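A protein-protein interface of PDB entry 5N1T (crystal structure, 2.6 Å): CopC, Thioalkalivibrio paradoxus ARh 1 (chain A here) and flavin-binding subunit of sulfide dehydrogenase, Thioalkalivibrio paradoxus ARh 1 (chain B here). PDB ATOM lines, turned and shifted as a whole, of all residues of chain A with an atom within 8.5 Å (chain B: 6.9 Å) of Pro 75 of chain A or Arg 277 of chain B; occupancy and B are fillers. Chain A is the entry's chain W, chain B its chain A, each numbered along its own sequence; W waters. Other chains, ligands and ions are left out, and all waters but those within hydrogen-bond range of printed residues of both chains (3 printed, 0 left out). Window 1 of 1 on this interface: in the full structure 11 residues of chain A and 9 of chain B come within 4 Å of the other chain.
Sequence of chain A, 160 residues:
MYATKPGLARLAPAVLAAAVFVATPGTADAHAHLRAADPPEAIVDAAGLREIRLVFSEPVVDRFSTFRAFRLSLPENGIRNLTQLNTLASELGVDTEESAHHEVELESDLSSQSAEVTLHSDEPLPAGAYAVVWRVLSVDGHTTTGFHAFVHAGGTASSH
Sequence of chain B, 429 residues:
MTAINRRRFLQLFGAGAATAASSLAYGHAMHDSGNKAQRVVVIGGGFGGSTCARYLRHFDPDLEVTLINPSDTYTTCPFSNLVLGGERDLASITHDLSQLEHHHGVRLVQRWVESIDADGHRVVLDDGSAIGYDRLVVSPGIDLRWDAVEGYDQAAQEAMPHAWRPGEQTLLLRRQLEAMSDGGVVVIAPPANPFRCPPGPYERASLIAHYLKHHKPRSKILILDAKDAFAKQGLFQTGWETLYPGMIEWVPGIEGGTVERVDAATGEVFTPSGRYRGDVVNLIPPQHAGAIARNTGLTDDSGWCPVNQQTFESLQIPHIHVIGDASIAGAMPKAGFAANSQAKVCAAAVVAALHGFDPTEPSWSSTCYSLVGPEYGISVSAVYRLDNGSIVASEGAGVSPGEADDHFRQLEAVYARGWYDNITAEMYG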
ATOM      1  N   LEU A  72      -9.465  -1.379  12.062  1.00  0.00           N
ATOM      2  CA  LEU A  72      -9.400  -2.447  11.038  1.00  0.00           C
ATOM      3  C   LEU A  72      -9.762  -1.884   9.657  1.00  0.00           C
ATOM      4  O   LEU A  72     -10.792  -1.199   9.521  1.00  0.00           O
ATOM      5  CB  LEU A  72     -10.312  -3.650  11.422  1.00  0.00           C
ATOM      6  CG  LEU A  72      -9.996  -4.390  12.756  1.00  0.00           C
ATOM      7  CD1 LEU A  72     -11.033  -5.458  13.131  1.00  0.00           C
ATOM      8  CD2 LEU A  72      -8.560  -4.945  12.758  1.00  0.00           C
ATOM      9  N   SER A  73      -8.905  -2.116   8.657  1.00  0.00           N
ATOM     10  CA  SER A  73      -9.258  -1.789   7.274  1.00  0.00           C
ATOM     11  C   SER A  73      -9.910  -2.999   6.651  1.00  0.00           C
ATOM     12  O   SER A  73      -9.241  -3.992   6.315  1.00  0.00           O
ATOM     13  CB  SER A  73      -8.072  -1.287   6.461  1.00  0.00           C
ATOM     14  OG  SER A  73      -6.955  -2.071   6.744  1.00  0.00           O
ATOM     15  N   LEU A  74     -11.230  -2.897   6.524  1.00  0.00           N
ATOM     16  CA  LEU A  74     -12.097  -4.011   6.166  1.00  0.00           C
ATOM     17  C   LEU A  74     -11.854  -4.505   4.728  1.00  0.00           C
ATOM     18  O   LEU A  74     -11.237  -3.807   3.947  1.00  0.00           O
ATOM     19  CB  LEU A  74     -13.561  -3.627   6.412  1.00  0.00           C
ATOM     20  CG  LEU A  74     -14.029  -3.325   7.856  1.00  0.00           C
ATOM     21  CD1 LEU A  74     -15.379  -2.619   7.802  1.00  0.00           C
ATOM     22  CD2 LEU A  74     -14.133  -4.581   8.724  1.00  0.00           C
ATOM     23  N   PRO A  75     -12.264  -5.739   4.393  1.00  0.00           N
ATOM     24  CA  PRO A  75     -12.181  -6.104   2.972  1.00  0.00           C
ATOM     25  C   PRO A  75     -13.024  -5.194   2.087  1.00  0.00           C
ATOM     26  O   PRO A  75     -14.012  -4.638   2.554  1.00  0.00           O
ATOM     27  CB  PRO A  75     -12.779  -7.513   2.947  1.00  0.00           C
ATOM     28  CG  PRO A  75     -13.411  -7.713   4.299  1.00  0.00           C
ATOM     29  CD  PRO A  75     -12.565  -6.915   5.217  1.00  0.00           C
ATOM     30  N   GLU A  76     -12.626  -5.041   0.829  1.00  0.00           N
ATOM     31  CA  GLU A  76     -13.417  -4.298  -0.179  1.00  0.00           C
ATOM     32  C   GLU A  76     -14.915  -4.569  -0.212  1.00  0.00           C
ATOM     33  O   GLU A  76     -15.674  -3.649  -0.449  1.00  0.00           O
ATOM     34  CB  GLU A  76     -12.883  -4.513  -1.594  1.00  0.00           C
ATOM     35  CG  GLU A  76     -11.504  -3.940  -1.814  1.00  0.00           C
ATOM     36  CD  GLU A  76     -11.433  -2.522  -1.339  1.00  0.00           C
ATOM     37  OE1 GLU A  76     -10.676  -2.272  -0.382  1.00  0.00           O
ATOM     38  OE2 GLU A  76     -12.173  -1.682  -1.902  1.00  0.00           O
ATOM     39  N   ASN A  77     -15.329  -5.818   0.010  1.00  0.00           N
ATOM     40  CA  ASN A  77     -16.752  -6.218  -0.063  1.00  0.00           C
ATOM     41  C   ASN A  77     -17.297  -6.446   1.359  1.00  0.00           C
ATOM     42  O   ASN A  77     -18.388  -7.001   1.560  1.00  0.00           O
ATOM     43  CB  ASN A  77     -16.879  -7.477  -0.931  1.00  0.00           C
ATOM     44  CG  ASN A  77     -16.097  -8.640  -0.369  1.00  0.00           C
ATOM     45  OD1 ASN A  77     -14.917  -8.525  -0.010  1.00  0.00           O
ATOM     46  ND2 ASN A  77     -16.754  -9.757  -0.250  1.00  0.00           N
ATOM     47  N   GLY A  78     -16.488  -6.035   2.340  1.00  0.00           N
ATOM     48  CA  GLY A  78     -16.877  -5.941   3.738  1.00  0.00           C
ATOM     49  C   GLY A  78     -17.132  -7.241   4.463  1.00  0.00           C
ATOM     50  O   GLY A  78     -17.038  -8.327   3.887  1.00  0.00           O
ATOM     51  N   ILE A  79     -17.496  -7.112   5.732  1.00  0.00           N
ATOM     52  CA  ILE A  79     -17.844  -8.246   6.542  1.00  0.00           C
ATOM     53  C   ILE A  79     -19.354  -8.264   6.770  1.00  0.00           C
ATOM     54  O   ILE A  79     -20.020  -7.245   6.628  1.00  0.00           O
ATOM     55  CB  ILE A  79     -17.033  -8.287   7.861  1.00  0.00           C
ATOM     56  CG1 ILE A  79     -17.420  -7.142   8.796  1.00  0.00           C
ATOM     57  CG2 ILE A  79     -15.523  -8.289   7.595  1.00  0.00           C
ATOM     58  CD1 ILE A  79     -16.779  -7.248  10.168  1.00  0.00           C
ATOM     59  N   ARG A  80     -19.874  -9.436   7.140  1.00  0.00           N
ATOM     60  CA  ARG A  80     -21.307  -9.695   7.237  1.00  0.00           C
ATOM     61  C   ARG A  80     -21.753 -10.035   8.643  1.00  0.00           C
ATOM     62  O   ARG A  80     -22.948 -10.044   8.924  1.00  0.00           O
ATOM     63  CB  ARG A  80     -21.714 -10.814   6.261  1.00  0.00           C
ATOM     64  CG  ARG A  80     -21.799 -10.350   4.797  1.00  0.00           C
ATOM     65  CD  ARG A  80     -22.294 -11.442   3.852  1.00  0.00           C
ATOM     66  NE  ARG A  80     -23.521 -12.074   4.345  1.00  0.00           N
ATOM     67  CZ  ARG A  80     -24.755 -11.567   4.216  1.00  0.00           C
ATOM     68  NH1 ARG A  80     -24.982 -10.400   3.587  1.00  0.00           N
ATOM     69  NH2 ARG A  80     -25.782 -12.245   4.719  1.00  0.00           N
ATOM     70  N   ASN A  81     -20.813 -10.313   9.532  1.00  0.00           N
ATOM     71  CA  ASN A  81     -21.143 -10.495  10.954  1.00  0.00           C
ATOM     72  C   ASN A  81     -19.917 -10.331  11.856  1.00  0.00           C
ATOM     73  O   ASN A  81     -18.817 -10.006  11.393  1.00  0.00           O
ATOM     74  CB  ASN A  81     -21.757 -11.883  11.178  1.00  0.00           C
ATOM     75  CG  ASN A  81     -20.884 -12.990  10.619  1.00  0.00           C
ATOM     76  OD1 ASN A  81     -19.652 -13.066  10.851  1.00  0.00           O
ATOM     77  ND2 ASN A  81     -21.506 -13.850   9.879  1.00  0.00           N
ATOM     78  N   THR A  83     -18.406 -12.736  13.698  1.00  0.00           N
ATOM     79  CA  THR A  83     -17.410 -13.812  13.603  1.00  0.00           C
ATOM     80  C   THR A  83     -16.274 -13.346  12.685  1.00  0.00           C
ATOM     81  O   THR A  83     -15.085 -13.531  12.994  1.00  0.00           O
ATOM     82  CB  THR A  83     -18.027 -15.183  13.165  1.00  0.00           C
ATOM     83  OG1 THR A  83     -19.061 -15.547  14.082  1.00  0.00           O
ATOM     84  CG2 THR A  83     -16.975 -16.322  13.159  1.00  0.00           C
ATOM     85  N   GLN A  84     -16.664 -12.700  11.592  1.00  0.00           N
ATOM     86  CA  GLN A  84     -15.719 -12.135  10.615  1.00  0.00           C
ATOM     87  C   GLN A  84     -14.952 -10.924  11.165  1.00  0.00           C
ATOM     88  O   GLN A  84     -13.779 -10.721  10.787  1.00  0.00           O
ATOM     89  CB  GLN A  84     -16.424 -11.817   9.280  1.00  0.00           C
ATOM     90  CG  GLN A  84     -17.080 -13.044   8.622  1.00  0.00           C
ATOM     91  CD  GLN A  84     -18.188 -12.698   7.628  1.00  0.00           C
ATOM     92  OE1 GLN A  84     -18.207 -11.622   7.028  1.00  0.00           O
ATOM     93  NE2 GLN A  84     -19.110 -13.627   7.438  1.00  0.00           N
ATOM     94  N   LEU A  85     -15.584 -10.144  12.060  1.00  0.00           N
ATOM     95  CA  LEU A  85     -14.859  -9.087  12.786  1.00  0.00           C
ATOM     96  C   LEU A  85     -13.725  -9.718  13.558  1.00  0.00           C
ATOM     97  O   LEU A  85     -12.552  -9.387  13.329  1.00  0.00           O
ATOM     98  CB  LEU A  85     -15.749  -8.257  13.724  1.00  0.00           C
ATOM     99  CG  LEU A  85     -15.112  -6.971  14.302  1.00  0.00           C
ATOM    100  CD1 LEU A  85     -14.490  -6.116  13.232  1.00  0.00           C
ATOM    101  CD2 LEU A  85     -16.061  -6.099  15.086  1.00  0.00           C
ATOM    102  N   THR A  87     -12.354 -12.838  13.368  1.00  0.00           N
ATOM    103  CA  THR A  87     -11.312 -13.475  12.589  1.00  0.00           C
ATOM    104  C   THR A  87     -10.287 -12.414  12.209  1.00  0.00           C
ATOM    105  O   THR A  87      -9.105 -12.569  12.480  1.00  0.00           O
ATOM    106  CB  THR A  87     -11.843 -14.128  11.304  1.00  0.00           C
ATOM    107  OG1 THR A  87     -12.938 -14.992  11.614  1.00  0.00           O
ATOM    108  CG2 THR A  87     -10.714 -14.892  10.555  1.00  0.00           C
ATOM    109  N   LEU A  88     -10.770 -11.324  11.616  1.00  0.00           N
ATOM    110  CA  LEU A  88      -9.917 -10.299  11.063  1.00  0.00           C
ATOM    111  C   LEU A  88      -9.107  -9.674  12.192  1.00  0.00           C
ATOM    112  O   LEU A  88      -7.885  -9.513  12.066  1.00  0.00           O
ATOM    113  CB  LEU A  88     -10.769  -9.281  10.290  1.00  0.00           C
ATOM    114  CG  LEU A  88     -10.221  -7.988   9.684  1.00  0.00           C
ATOM    115  CD1 LEU A  88      -8.912  -8.221   8.951  1.00  0.00           C
ATOM    116  CD2 LEU A  88     -11.257  -7.383   8.746  1.00  0.00           C
ATOM    117  N   HIS A 101      -3.582  -2.790   8.951  1.00  0.00           N
ATOM    118  CA  HIS A 101      -4.381  -1.941   9.806  1.00  0.00           C
ATOM    119  C   HIS A 101      -3.617  -0.700  10.346  1.00  0.00           C
ATOM    120  O   HIS A 101      -2.403  -0.549  10.129  1.00  0.00           O
ATOM    121  CB  HIS A 101      -5.040  -2.811  10.871  1.00  0.00           C
ATOM    122  CG  HIS A 101      -5.692  -4.040  10.307  1.00  0.00           C
ATOM    123  ND1 HIS A 101      -6.785  -3.984   9.476  1.00  0.00           N
ATOM    124  CD2 HIS A 101      -5.389  -5.355  10.427  1.00  0.00           C
ATOM    125  CE1 HIS A 101      -7.143  -5.209   9.124  1.00  0.00           C
ATOM    126  NE2 HIS A 101      -6.310  -6.058   9.688  1.00  0.00           N
ATOM    127  N   ALA A 129     -14.268  -0.279  12.363  1.00  0.00           N
ATOM    128  CA  ALA A 129     -14.076  -1.525  13.101  1.00  0.00           C
ATOM    129  C   ALA A 129     -12.748  -1.396  13.836  1.00  0.00           C
ATOM    130  O   ALA A 129     -11.726  -1.048  13.231  1.00  0.00           O
ATOM    131  CB  ALA A 129     -14.022  -2.712  12.153  1.00  0.00           C
ATOM    132  N   GLY B 183     -27.062 -15.149   1.134  1.00  0.00           N
ATOM    133  CA  GLY B 183     -26.527 -13.804   1.291  1.00  0.00           C
ATOM    134  C   GLY B 183     -25.023 -13.761   1.230  1.00  0.00           C
ATOM    135  O   GLY B 183     -24.465 -12.678   1.128  1.00  0.00           O
ATOM    136  N   GLY B 184     -24.380 -14.934   1.279  1.00  0.00           N
ATOM    137  CA  GLY B 184     -22.920 -15.063   1.130  1.00  0.00           C
ATOM    138  C   GLY B 184     -22.383 -14.817  -0.280  1.00  0.00           C
ATOM    139  O   GLY B 184     -23.156 -14.716  -1.266  1.00  0.00           O
ATOM    140  N   VAL B 185     -21.052 -14.766  -0.358  1.00  0.00           N
ATOM    141  CA  VAL B 185     -20.306 -14.391  -1.553  1.00  0.00           C
ATOM    142  C   VAL B 185     -19.416 -15.564  -1.938  1.00  0.00           C
ATOM    143  O   VAL B 185     -18.544 -15.981  -1.149  1.00  0.00           O
ATOM    144  CB  VAL B 185     -19.365 -13.166  -1.303  1.00  0.00           C
ATOM    145  CG1 VAL B 185     -18.818 -12.627  -2.612  1.00  0.00           C
ATOM    146  CG2 VAL B 185     -20.068 -12.035  -0.564  1.00  0.00           C
ATOM    147  N   VAL B 186     -19.621 -16.090  -3.139  1.00  0.00           N
ATOM    148  CA  VAL B 186     -18.735 -17.117  -3.718  1.00  0.00           C
ATOM    149  C   VAL B 186     -17.676 -16.416  -4.543  1.00  0.00           C
ATOM    150  O   VAL B 186     -18.004 -15.609  -5.395  1.00  0.00           O
ATOM    151  CB  VAL B 186     -19.513 -18.076  -4.646  1.00  0.00           C
ATOM    152  CG1 VAL B 186     -18.669 -19.299  -4.985  1.00  0.00           C
ATOM    153  CG2 VAL B 186     -20.834 -18.492  -4.000  1.00  0.00           C
ATOM    154  N   VAL B 187     -16.413 -16.724  -4.310  1.00  0.00           N
ATOM    155  CA  VAL B 187     -15.337 -16.073  -5.052  1.00  0.00           C
ATOM    156  C   VAL B 187     -14.709 -17.115  -5.959  1.00  0.00           C
ATOM    157  O   VAL B 187     -14.375 -18.237  -5.512  1.00  0.00           O
ATOM    158  CB  VAL B 187     -14.264 -15.500  -4.126  1.00  0.00           C
ATOM    159  CG1 VAL B 187     -13.092 -14.963  -4.918  1.00  0.00           C
ATOM    160  CG2 VAL B 187     -14.829 -14.413  -3.221  1.00  0.00           C
ATOM    161  N   LEU B 222     -18.464 -13.352  -7.341  1.00  0.00           N
ATOM    162  CA  LEU B 222     -17.413 -12.403  -7.577  1.00  0.00           C
ATOM    163  C   LEU B 222     -16.224 -13.108  -8.260  1.00  0.00           C
ATOM    164  O   LEU B 222     -15.565 -13.939  -7.652  1.00  0.00           O
ATOM    165  CB  LEU B 222     -16.923 -11.798  -6.223  1.00  0.00           C
ATOM    166  CG  LEU B 222     -15.822 -10.748  -6.436  1.00  0.00           C
ATOM    167  CD1 LEU B 222     -16.304  -9.616  -7.352  1.00  0.00           C
ATOM    168  CD2 LEU B 222     -15.274 -10.219  -5.140  1.00  0.00           C
ATOM    169  N   THR B 266      -8.529 -17.990   6.434  1.00  0.00           N
ATOM    170  CA  THR B 266      -9.563 -16.938   6.579  1.00  0.00           C
ATOM    171  C   THR B 266     -10.540 -16.644   5.388  1.00  0.00           C
ATOM    172  O   THR B 266     -11.349 -15.720   5.466  1.00  0.00           O
ATOM    173  CB  THR B 266      -8.926 -15.633   7.098  1.00  0.00           C
ATOM    174  OG1 THR B 266      -8.120 -15.037   6.065  1.00  0.00           O
ATOM    175  CG2 THR B 266      -8.055 -15.919   8.297  1.00  0.00           C
ATOM    176  N   GLY B 267     -10.482 -17.416   4.299  1.00  0.00           N
ATOM    177  CA  GLY B 267     -11.322 -17.148   3.107  1.00  0.00           C
ATOM    178  C   GLY B 267     -11.050 -15.781   2.474  1.00  0.00           C
ATOM    179  O   GLY B 267     -11.968 -15.077   2.020  1.00  0.00           O
ATOM    180  N   GLU B 268      -9.769 -15.420   2.443  1.00  0.00           N
ATOM    181  CA  GLU B 268      -9.369 -14.116   2.017  1.00  0.00           C
ATOM    182  C   GLU B 268      -8.458 -14.212   0.839  1.00  0.00           C
ATOM    183  O   GLU B 268      -7.580 -15.070   0.780  1.00  0.00           O
ATOM    184  CB  GLU B 268      -8.723 -13.364   3.158  1.00  0.00           C
ATOM    185  CG  GLU B 268      -9.781 -12.831   4.113  1.00  0.00           C
ATOM    186  CD  GLU B 268      -9.229 -12.035   5.277  1.00  0.00           C
ATOM    187  OE1 GLU B 268      -8.277 -12.522   5.947  1.00  0.00           O
ATOM    188  OE2 GLU B 268      -9.782 -10.928   5.520  1.00  0.00           O
ATOM    189  N   VAL B 269      -8.710 -13.323  -0.109  1.00  0.00           N
ATOM    190  CA  VAL B 269      -7.994 -13.263  -1.348  1.00  0.00           C
ATOM    191  C   VAL B 269      -7.443 -11.844  -1.423  1.00  0.00           C
ATOM    192  O   VAL B 269      -8.118 -10.887  -1.030  1.00  0.00           O
ATOM    193  CB  VAL B 269      -8.964 -13.620  -2.481  1.00  0.00           C
ATOM    194  CG1 VAL B 269      -8.440 -13.168  -3.820  1.00  0.00           C
ATOM    195  CG2 VAL B 269      -9.136 -15.134  -2.543  1.00  0.00           C
ATOM    196  N   GLY B 274      -7.225  -4.568  -3.573  1.00  0.00           N
ATOM    197  CA  GLY B 274      -7.639  -4.817  -2.208  1.00  0.00           C
ATOM    198  C   GLY B 274      -7.817  -6.253  -1.823  1.00  0.00           C
ATOM    199  O   GLY B 274      -7.576  -7.183  -2.610  1.00  0.00           O
ATOM    200  N   ARG B 275      -8.232  -6.400  -0.579  1.00  0.00           N
ATOM    201  CA  ARG B 275      -8.462  -7.658   0.084  1.00  0.00           C
ATOM    202  C   ARG B 275      -9.976  -7.969  -0.083  1.00  0.00           C
ATOM    203  O   ARG B 275     -10.798  -7.080  -0.018  1.00  0.00           O
ATOM    204  CB  ARG B 275      -7.956  -7.500   1.539  1.00  0.00           C
ATOM    205  CG  ARG B 275      -8.491  -8.445   2.620  1.00  0.00           C
ATOM    206  CD  ARG B 275      -8.272  -7.852   4.028  1.00  0.00           C
ATOM    207  NE  ARG B 275      -7.996  -8.925   4.969  1.00  0.00           N
ATOM    208  CZ  ARG B 275      -7.088  -8.899   5.950  1.00  0.00           C
ATOM    209  NH1 ARG B 275      -6.320  -7.827   6.209  1.00  0.00           N
ATOM    210  NH2 ARG B 275      -6.938  -9.987   6.682  1.00  0.00           N
ATOM    211  N   TYR B 276     -10.328  -9.215  -0.370  1.00  0.00           N
ATOM    212  CA  TYR B 276     -11.749  -9.638  -0.457  1.00  0.00           C
ATOM    213  C   TYR B 276     -11.951 -10.867   0.382  1.00  0.00           C
ATOM    214  O   TYR B 276     -11.009 -11.653   0.562  1.00  0.00           O
ATOM    215  CB  TYR B 276     -12.132 -10.019  -1.879  1.00  0.00           C
ATOM    216  CG  TYR B 276     -11.978  -8.912  -2.855  1.00  0.00           C
ATOM    217  CD1 TYR B 276     -10.742  -8.680  -3.495  1.00  0.00           C
ATOM    218  CD2 TYR B 276     -13.069  -8.103  -3.170  1.00  0.00           C
ATOM    219  CE1 TYR B 276     -10.602  -7.655  -4.404  1.00  0.00           C
ATOM    220  CE2 TYR B 276     -12.950  -7.076  -4.082  1.00  0.00           C
ATOM    221  CZ  TYR B 276     -11.720  -6.868  -4.676  1.00  0.00           C
ATOM    222  OH  TYR B 276     -11.612  -5.852  -5.546  1.00  0.00           O
ATOM    223  N   ARG B 277     -13.152 -11.053   0.901  1.00  0.00           N
ATOM    224  CA  ARG B 277     -13.407 -12.293   1.605  1.00  0.00           C
ATOM    225  C   ARG B 277     -14.559 -13.043   1.025  1.00  0.00           C
ATOM    226  O   ARG B 277     -15.570 -12.463   0.657  1.00  0.00           O
ATOM    227  CB  ARG B 277     -13.566 -12.124   3.111  1.00  0.00           C
ATOM    228  CG  ARG B 277     -14.648 -11.185   3.516  1.00  0.00           C
ATOM    229  CD  ARG B 277     -15.485 -11.748   4.646  1.00  0.00           C
ATOM    230  NE  ARG B 277     -16.818 -11.542   4.138  1.00  0.00           N
ATOM    231  CZ  ARG B 277     -17.711 -12.483   3.937  1.00  0.00           C
ATOM    232  NH1 ARG B 277     -18.873 -12.137   3.404  1.00  0.00           N
ATOM    233  NH2 ARG B 277     -17.462 -13.735   4.302  1.00  0.00           N
ATOM    234  N   GLY B 278     -14.381 -14.342   0.938  1.00  0.00           N
ATOM    235  CA  GLY B 278     -15.402 -15.166   0.395  1.00  0.00           C
ATOM    236  C   GLY B 278     -15.875 -16.115   1.449  1.00  0.00           C
ATOM    237  O   GLY B 278     -15.052 -16.645   2.217  1.00  0.00           O
ATOM    238  N   ASP B 279     -17.196 -16.336   1.476  1.00  0.00           N
ATOM    239  CA  ASP B 279     -17.785 -17.362   2.323  1.00  0.00           C
ATOM    240  C   ASP B 279     -17.450 -18.732   1.775  1.00  0.00           C
ATOM    241  O   ASP B 279     -17.310 -19.695   2.523  1.00  0.00           O
ATOM    242  CB  ASP B 279     -19.264 -17.172   2.396  1.00  0.00           C
ATOM    243  CG  ASP B 279     -19.626 -15.875   3.033  1.00  0.00           C
ATOM    244  OD1 ASP B 279     -19.677 -14.867   2.308  1.00  0.00           O
ATOM    245  OD2 ASP B 279     -19.848 -15.860   4.263  1.00  0.00           O
ATOM    246  N   VAL B 280     -17.327 -18.791   0.452  1.00  0.00           N
ATOM    247  CA  VAL B 280     -16.757 -19.912  -0.271  1.00  0.00           C
ATOM    248  C   VAL B 280     -15.797 -19.275  -1.269  1.00  0.00           C
ATOM    249  O   VAL B 280     -16.129 -18.272  -1.894  1.00  0.00           O
ATOM    250  CB  VAL B 280     -17.818 -20.730  -1.054  1.00  0.00           C
ATOM    251  CG1 VAL B 280     -17.178 -21.935  -1.732  1.00  0.00           C
ATOM    252  CG2 VAL B 280     -18.964 -21.179  -0.145  1.00  0.00           C
ATOM    253  N   VAL B 281     -14.595 -19.834  -1.394  1.00  0.00           N
ATOM    254  CA  VAL B 281     -13.711 -19.415  -2.455  1.00  0.00           C
ATOM    255  C   VAL B 281     -13.106 -20.544  -3.243  1.00  0.00           C
ATOM    256  O   VAL B 281     -12.488 -21.472  -2.702  1.00  0.00           O
ATOM    257  CB  VAL B 281     -12.712 -18.292  -2.073  1.00  0.00           C
ATOM    258  CG1 VAL B 281     -12.848 -17.886  -0.617  1.00  0.00           C
ATOM    259  CG2 VAL B 281     -11.278 -18.578  -2.530  1.00  0.00           C
HETATM  260  O   HOH W   1      -8.895  -3.871   0.718  1.00  0.00           O
HETATM  261  O   HOH W   2     -21.770 -14.364   5.432  1.00  0.00           O
HETATM  262  O   HOH W   3     -19.761  -9.607   2.320  1.00  0.00           O
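O of Arg 275 of chain B lies within hydrogen-bond range of N of Glu 76 of chain A, at 2.9 Å. The side-chain amide oxygen (OE1) of Gln 84 of chain A sits at hydrogen-bond distance from the guanidinium group (NE) of Arg 277 of chain B (3.2 Å). NE of Arg 277 of chain B sits at hydrogen-bond distance from O of Gly 78 of chain A (3.2 Å). O of Gly 183 of chain B lies close to NH1 of Arg 80 of chain A, at 3.4 Å. The side-chain amide nitrogen (ND2) of Asn 77 of chain A sits at hydrogen-bond distance from the backbone carbonyl oxygen (O) of Arg 277 of chain B, 3.1 Å away.
O of Thr 83 of chain A sits at hydrogen-bond distance from OG1 of Thr 87 of chain A (2.9 Å). The side-chain carboxylate (OE1) of Glu 268 of chain B lies within hydrogen-bond range of the side-chain hydroxyl (OG1) of Thr 266 of chain B (2.5 Å). OE2 of Glu 268 of chain B is in salt-bridge range of NE of Arg 275 of chain B, at 2.7 Å. The backbone NH (N) of Gln 84 of chain A is in hydrogen-bond range of the side-chain amide oxygen (OD1) of Asn 81 of chain A (3.1 Å). The backbone NH (N) of Ser 73 of chain A sits at hydrogen-bond distance from a ring nitrogen (ND1) of His 101 of chain A (2.9 Å). NH1 of Arg 277 of chain B lies within salt-bridge range of OD1 of Asp 279 of chain B (3.0 Å).
Pro 75 of chain A touches Arg 275 of chain B (CA to O, 3.4 Å). CG of Arg 277 of chain B touches CG of Pro 75 of chain A (3.8 Å). Glu 76 of chain A touches Gly 274 of chain B. Tyr 276 of chain B touches Glu 76 of chain A (CE2 to CB, 3.6 Å). Asn 77 of chain A touches Tyr 276 of chain B. NH1 of Arg 277 of chain B touches CD of Arg 80 of chain A, 3.5 Å away. Gln 84 of chain A touches Asp 279 of chain B (NE2 to OD2, 3.95 Å). CG2 of Thr 87 of chain A touches CG2 of Thr 266 of chain B, at 3.6 Å. Leu 88 of chain A touches Arg 275 of chain B. His 101 of chain A touches Arg 275 of chain B.
Of chain B, only Arg 275 and Arg 277 come within 4 Å of Pro 75 of chain A. Printed residues of chain A within 4 Å of Arg 277 of chain B: Pro 75 (3.8 Å), Asn 77 (3.1 Å), Gly 78 (3.2 Å), Arg 80 (3.5 Å) and Gln 84 (3.2 Å). Of the printed residues of chain B, Gly 78 of chain A touches Arg 277 (3.2 Å). Printed residues of chain A within 4 Å of Thr 266 of chain B: Thr 87 (3.6 Å). Of the printed residues of chain B, His 101 of chain A touches Arg 275. Printed residues of chain B within 4 Å of Asn 77 of chain A: Tyr 276 and Arg 277. Of the printed residues of chain B, Arg 80 of chain A touches Gly 183 and Arg 277. The nearest residue of chain B that does not touch Pro 75 of chain A is Tyr 276 of chain B (4.1 Å).
Water W1 lies within hydrogen-bond range of OE1 of Glu 76 of chain A (2.6 Å) and N of Arg 275 of chain B (2.9 Å). Water W2 lies within hydrogen-bond range of OD2 of Asp 279 of chain B (2.7 Å), NE of Arg 80 of chain A (3.1 Å) and NE2 of Gln 84 of chain A (3.4 Å). Water W3 lies within hydrogen-bond range of NH1 of Arg 277 of chain B (2.9 Å), O of Asn 77 of chain A (3.0 Å) and O of Gly 78 of chain A (3.4 Å).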
